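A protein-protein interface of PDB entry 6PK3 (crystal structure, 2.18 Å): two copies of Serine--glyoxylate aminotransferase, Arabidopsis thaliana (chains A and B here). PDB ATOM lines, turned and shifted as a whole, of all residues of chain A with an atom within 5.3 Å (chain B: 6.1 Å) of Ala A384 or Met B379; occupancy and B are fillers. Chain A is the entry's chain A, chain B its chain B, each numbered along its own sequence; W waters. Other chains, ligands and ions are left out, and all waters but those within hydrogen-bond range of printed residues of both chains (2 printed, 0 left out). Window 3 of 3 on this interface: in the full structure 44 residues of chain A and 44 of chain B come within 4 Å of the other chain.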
ATOM      1  N   GLY A 380      16.133 -32.333  27.819  1.00  0.00           N
ATOM      2  CA  GLY A 380      16.797 -31.052  27.736  1.00  0.00           C
ATOM      3  C   GLY A 380      18.308 -31.115  27.672  1.00  0.00           C
ATOM      4  O   GLY A 380      18.943 -30.086  27.407  1.00  0.00           O
ATOM      5  N   SER A 381      18.905 -32.290  27.888  1.00  0.00           N
ATOM      6  CA  SER A 381      20.361 -32.380  27.948  1.00  0.00           C
ATOM      7  C   SER A 381      20.997 -32.066  26.599  1.00  0.00           C
ATOM      8  O   SER A 381      22.021 -31.375  26.538  1.00  0.00           O
ATOM      9  CB  SER A 381      20.779 -33.771  28.425  1.00  0.00           C
ATOM     10  OG  SER A 381      20.299 -34.774  27.547  1.00  0.00           O
ATOM     11  N   GLY A 382      20.412 -32.570  25.510  1.00  0.00           N
ATOM     12  CA  GLY A 382      20.954 -32.279  24.193  1.00  0.00           C
ATOM     13  C   GLY A 382      20.657 -30.860  23.744  1.00  0.00           C
ATOM     14  O   GLY A 382      21.530 -30.175  23.203  1.00  0.00           O
ATOM     15  N   VAL A 383      19.423 -30.403  23.951  1.00  0.00           N
ATOM     16  CA  VAL A 383      19.094 -29.014  23.643  1.00  0.00           C
ATOM     17  C   VAL A 383      20.039 -28.077  24.384  1.00  0.00           C
ATOM     18  O   VAL A 383      20.564 -27.117  23.807  1.00  0.00           O
ATOM     19  CB  VAL A 383      17.621 -28.720  23.990  1.00  0.00           C
ATOM     20  CG1 VAL A 383      17.296 -27.249  23.748  1.00  0.00           C
ATOM     21  CG2 VAL A 383      16.692 -29.610  23.180  1.00  0.00           C
ATOM     22  N   ALA A 384      20.287 -28.355  25.667  1.00  0.00           N
ATOM     23  CA  ALA A 384      21.147 -27.485  26.460  1.00  0.00           C
ATOM     24  C   ALA A 384      22.578 -27.485  25.937  1.00  0.00           C
ATOM     25  O   ALA A 384      23.236 -26.439  25.907  1.00  0.00           O
ATOM     26  CB  ALA A 384      21.121 -27.917  27.926  1.00  0.00           C
ATOM     27  N   ALA A 385      23.086 -28.652  25.537  1.00  0.00           N
ATOM     28  CA  ALA A 385      24.444 -28.712  25.012  1.00  0.00           C
ATOM     29  C   ALA A 385      24.559 -27.927  23.712  1.00  0.00           C
ATOM     30  O   ALA A 385      25.582 -27.281  23.452  1.00  0.00           O
ATOM     31  CB  ALA A 385      24.866 -30.167  24.803  1.00  0.00           C
ATOM     32  N   ALA A 386      23.514 -27.961  22.886  1.00  0.00           N
ATOM     33  CA  ALA A 386      23.544 -27.228  21.628  1.00  0.00           C
ATOM     34  C   ALA A 386      23.351 -25.732  21.855  1.00  0.00           C
ATOM     35  O   ALA A 386      24.096 -24.911  21.307  1.00  0.00           O
ATOM     36  CB  ALA A 386      22.472 -27.772  20.681  1.00  0.00           C
ATOM     37  N   SER A 387      22.362 -25.356  22.670  1.00  0.00           N
ATOM     38  CA  SER A 387      22.092 -23.936  22.886  1.00  0.00           C
ATOM     39  C   SER A 387      23.219 -23.260  23.656  1.00  0.00           C
ATOM     40  O   SER A 387      23.500 -22.078  23.428  1.00  0.00           O
ATOM     41  CB  SER A 387      20.759 -23.756  23.617  1.00  0.00           C
ATOM     42  OG  SER A 387      20.764 -24.403  24.877  1.00  0.00           O
ATOM     43  N   THR A 388      23.877 -23.985  24.563  1.00  0.00           N
ATOM     44  CA  THR A 388      25.013 -23.411  25.276  1.00  0.00           C
ATOM     45  C   THR A 388      26.146 -23.074  24.315  1.00  0.00           C
ATOM     46  O   THR A 388      26.781 -22.019  24.434  1.00  0.00           O
ATOM     47  CB  THR A 388      25.498 -24.376  26.358  1.00  0.00           C
ATOM     48  OG1 THR A 388      24.466 -24.561  27.333  1.00  0.00           O
ATOM     49  CG2 THR A 388      26.748 -23.836  27.040  1.00  0.00           C
ATOM     50  N   TYR A 389      26.410 -23.960  23.352  1.00  0.00           N
ATOM     51  CA  TYR A 389      27.442 -23.696  22.356  1.00  0.00           C
ATOM     52  C   TYR A 389      27.011 -22.587  21.402  1.00  0.00           C
ATOM     53  O   TYR A 389      27.785 -21.668  21.110  1.00  0.00           O
ATOM     54  CB  TYR A 389      27.761 -24.981  21.588  1.00  0.00           C
ATOM     55  CG  TYR A 389      28.468 -24.748  20.275  1.00  0.00           C
ATOM     56  CD1 TYR A 389      29.843 -24.581  20.226  1.00  0.00           C
ATOM     57  CD2 TYR A 389      27.757 -24.692  19.084  1.00  0.00           C
ATOM     58  CE1 TYR A 389      30.493 -24.364  19.029  1.00  0.00           C
ATOM     59  CE2 TYR A 389      28.398 -24.475  17.881  1.00  0.00           C
ATOM     60  CZ  TYR A 389      29.766 -24.310  17.861  1.00  0.00           C
ATOM     61  OH  TYR A 389      30.410 -24.092  16.669  1.00  0.00           O
ATOM     62  N   GLN A 391      24.885 -20.120  21.755  1.00  0.00           N
ATOM     63  CA  GLN A 391      24.778 -18.788  22.338  1.00  0.00           C
ATOM     64  C   GLN A 391      26.092 -18.017  22.263  1.00  0.00           C
ATOM     65  O   GLN A 391      26.079 -16.785  22.360  1.00  0.00           O
ATOM     66  CB  GLN A 391      24.307 -18.898  23.789  1.00  0.00           C
ATOM     67  CG  GLN A 391      24.006 -17.562  24.457  1.00  0.00           C
ATOM     68  CD  GLN A 391      25.184 -17.012  25.234  1.00  0.00           C
ATOM     69  OE1 GLN A 391      26.118 -17.742  25.566  1.00  0.00           O
ATOM     70  NE2 GLN A 391      25.145 -15.718  25.531  1.00  0.00           N
ATOM     71  N   ALA B 364      13.595 -22.555  23.401  1.00  0.00           N
ATOM     72  CA  ALA B 364      15.045 -22.714  23.422  1.00  0.00           C
ATOM     73  C   ALA B 364      15.742 -21.404  23.079  1.00  0.00           C
ATOM     74  O   ALA B 364      16.779 -21.069  23.664  1.00  0.00           O
ATOM     75  CB  ALA B 364      15.467 -23.815  22.450  1.00  0.00           C
ATOM     76  N   GLU B 367      15.784 -18.892  26.034  1.00  0.00           N
ATOM     77  CA  GLU B 367      16.820 -19.197  27.015  1.00  0.00           C
ATOM     78  C   GLU B 367      18.150 -18.573  26.616  1.00  0.00           C
ATOM     79  O   GLU B 367      18.861 -18.012  27.459  1.00  0.00           O
ATOM     80  CB  GLU B 367      16.964 -20.712  27.177  1.00  0.00           C
ATOM     81  CG  GLU B 367      15.699 -21.398  27.670  1.00  0.00           C
ATOM     82  CD  GLU B 367      15.920 -22.849  28.062  1.00  0.00           C
ATOM     83  OE1 GLU B 367      16.934 -23.444  27.632  1.00  0.00           O
ATOM     84  OE2 GLU B 367      15.076 -23.391  28.806  1.00  0.00           O
ATOM     85  N   MET B 368      18.502 -18.654  25.331  1.00  0.00           N
ATOM     86  CA  MET B 368      19.745 -18.044  24.870  1.00  0.00           C
ATOM     87  C   MET B 368      19.693 -16.527  25.003  1.00  0.00           C
ATOM     88  O   MET B 368      20.700 -15.893  25.341  1.00  0.00           O
ATOM     89  CB  MET B 368      20.025 -18.453  23.424  1.00  0.00           C
ATOM     90  CG  MET B 368      20.345 -19.933  23.251  1.00  0.00           C
ATOM     91  SD  MET B 368      20.922 -20.360  21.591  1.00  0.00           S
ATOM     92  CE  MET B 368      19.433 -20.093  20.634  1.00  0.00           C
ATOM     93  N   LYS B 371      20.256 -15.456  28.562  1.00  0.00           N
ATOM     94  CA  LYS B 371      21.686 -15.471  28.848  1.00  0.00           C
ATOM     95  C   LYS B 371      22.373 -14.241  28.265  1.00  0.00           C
ATOM     96  O   LYS B 371      23.257 -13.656  28.903  1.00  0.00           O
ATOM     97  CB  LYS B 371      22.315 -16.751  28.299  1.00  0.00           C
ATOM     98  CG  LYS B 371      23.786 -16.903  28.647  1.00  0.00           C
ATOM     99  CD  LYS B 371      24.104 -18.296  29.167  1.00  0.00           C
ATOM    100  CE  LYS B 371      25.410 -18.310  29.949  1.00  0.00           C
ATOM    101  NZ  LYS B 371      26.447 -19.170  29.311  1.00  0.00           N
ATOM    102  N   VAL B 377      19.940 -17.981  33.697  1.00  0.00           N
ATOM    103  CA  VAL B 377      19.091 -19.100  33.316  1.00  0.00           C
ATOM    104  C   VAL B 377      19.930 -20.369  33.228  1.00  0.00           C
ATOM    105  O   VAL B 377      21.106 -20.341  32.853  1.00  0.00           O
ATOM    106  CB  VAL B 377      18.379 -18.799  31.981  1.00  0.00           C
ATOM    107  CG1 VAL B 377      19.386 -18.751  30.841  1.00  0.00           C
ATOM    108  CG2 VAL B 377      17.301 -19.830  31.704  1.00  0.00           C
ATOM    109  N   VAL B 378      19.322 -21.496  33.586  1.00  0.00           N
ATOM    110  CA  VAL B 378      19.933 -22.806  33.393  1.00  0.00           C
ATOM    111  C   VAL B 378      19.514 -23.297  32.011  1.00  0.00           C
ATOM    112  O   VAL B 378      18.334 -23.563  31.769  1.00  0.00           O
ATOM    113  CB  VAL B 378      19.517 -23.794  34.489  1.00  0.00           C
ATOM    114  CG1 VAL B 378      20.168 -25.155  34.249  1.00  0.00           C
ATOM    115  CG2 VAL B 378      19.888 -23.253  35.864  1.00  0.00           C
ATOM    116  N   MET B 379      20.479 -23.409  31.100  1.00  0.00           N
ATOM    117  CA  MET B 379      20.166 -23.772  29.724  1.00  0.00           C
ATOM    118  C   MET B 379      19.477 -25.130  29.679  1.00  0.00           C
ATOM    119  O   MET B 379      19.962 -26.108  30.256  1.00  0.00           O
ATOM    120  CB  MET B 379      21.440 -23.796  28.878  1.00  0.00           C
ATOM    121  CG  MET B 379      22.193 -22.476  28.838  1.00  0.00           C
ATOM    122  SD  MET B 379      21.167 -21.060  28.399  1.00  0.00           S
ATOM    123  CE  MET B 379      21.030 -21.230  26.629  1.00  0.00           C
ATOM    124  N   GLY B 380      18.335 -25.184  28.993  1.00  0.00           N
ATOM    125  CA  GLY B 380      17.571 -26.402  28.852  1.00  0.00           C
ATOM    126  C   GLY B 380      16.519 -26.629  29.918  1.00  0.00           C
ATOM    127  O   GLY B 380      15.650 -27.491  29.729  1.00  0.00           O
ATOM    128  N   SER B 381      16.564 -25.884  31.025  1.00  0.00           N
ATOM    129  CA  SER B 381      15.624 -26.120  32.118  1.00  0.00           C
ATOM    130  C   SER B 381      14.183 -25.884  31.680  1.00  0.00           C
ATOM    131  O   SER B 381      13.284 -26.652  32.040  1.00  0.00           O
ATOM    132  CB  SER B 381      15.971 -25.222  33.306  1.00  0.00           C
ATOM    133  OG  SER B 381      15.883 -23.853  32.952  1.00  0.00           O
ATOM    134  N   GLY B 382      13.939 -24.819  30.913  1.00  0.00           N
ATOM    135  CA  GLY B 382      12.582 -24.543  30.467  1.00  0.00           C
ATOM    136  C   GLY B 382      12.127 -25.478  29.363  1.00  0.00           C
ATOM    137  O   GLY B 382      10.956 -25.863  29.307  1.00  0.00           O
HETATM  138  O   HOH W   1      26.485 -20.147  26.487  1.00  0.00           O
HETATM  139  O   HOH W   2      17.974 -23.431  25.019  1.00  0.00           O
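The backbone carbonyl oxygen of Ser A387 sits close to the side-chain sulfur of Met B368, at 3.6 Å.
O of Val A383 sits at hydrogen-bond distance from OG of Ser A387, 2.9 Å away. OG of Ser A387 lies within hydrogen-bond range of O of Ala A384 (3.4 Å). The backbone carbonyl oxygen (O) of Ala A384 sits at hydrogen-bond distance from the side-chain hydroxyl (OG1) of Thr A388, 2.7 Å away. The backbone NH (N) of Gly B380 lies within hydrogen-bond range of the side-chain carboxylate (OE1) of Glu B367 (2.6 Å).
Among the printed residues, pairs that only touch across the chains: Ala A384 with Met B379, Ala A384 with Gly B380, Ser A387 with Met B379, Thr A388 with Met B379, Gln A391 with Met B368 and Gln A391 with Lys B371.
Of chain B, only Met B379 (3.2 Å) and Gly B380 (3.97 Å) come within 4 Å of Ala A384. Of the printed residues of chain B, Ser A387 touches Met B368 and Met B379. Printed residues of chain B within 4 Å of Gln A391: Met B368 (3.8 Å) and Lys B371 (3.6 Å). Of the printed residues of chain A, Met B368 touches Ser A387 (3.6 Å) and Gln A391 (3.8 Å). Of the printed residues of chain A, Lys B371 touches Gln A391 (3.6 Å). Val B377 touches none of the printed residues of chain A. The nearest residue of chain B that does not touch Ala A384 is Ser B381 (5.9 Å). The nearest printed residue of chain A that does not touch Lys B371 is Thr A388 (5.2 Å).
Of the 10 printed residues of chain B, 4 touch a printed residue of chain A. Printed residues of chain B that touch a printed residue of chain A: Met B368, Lys B371, Met B379 and Gly B380. Hydrophobic or aromatic side chains of chain B that line the printed part of chain A: Met B368 and Met B379. Among the printed residues, no Asp or Glu carboxylate lies within 4 Å of a Lys or Arg side-chain nitrogen of the other chain.
3 positions are printed for both chains.
Water W1 lies within hydrogen-bond range of the side-chain amide oxygen of Gln A391 (2.6 Å), the backbone carbonyl oxygen of Thr A388 (2.8 Å) and the side-chain amino group of Lys B371 (3.0 Å). Water W2 lies within hydrogen-bond range of OE1 of Glu B367 (2.8 Å), OG of Ser A387 (3.0 Å) and O of Ala B364 (3.0 Å).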
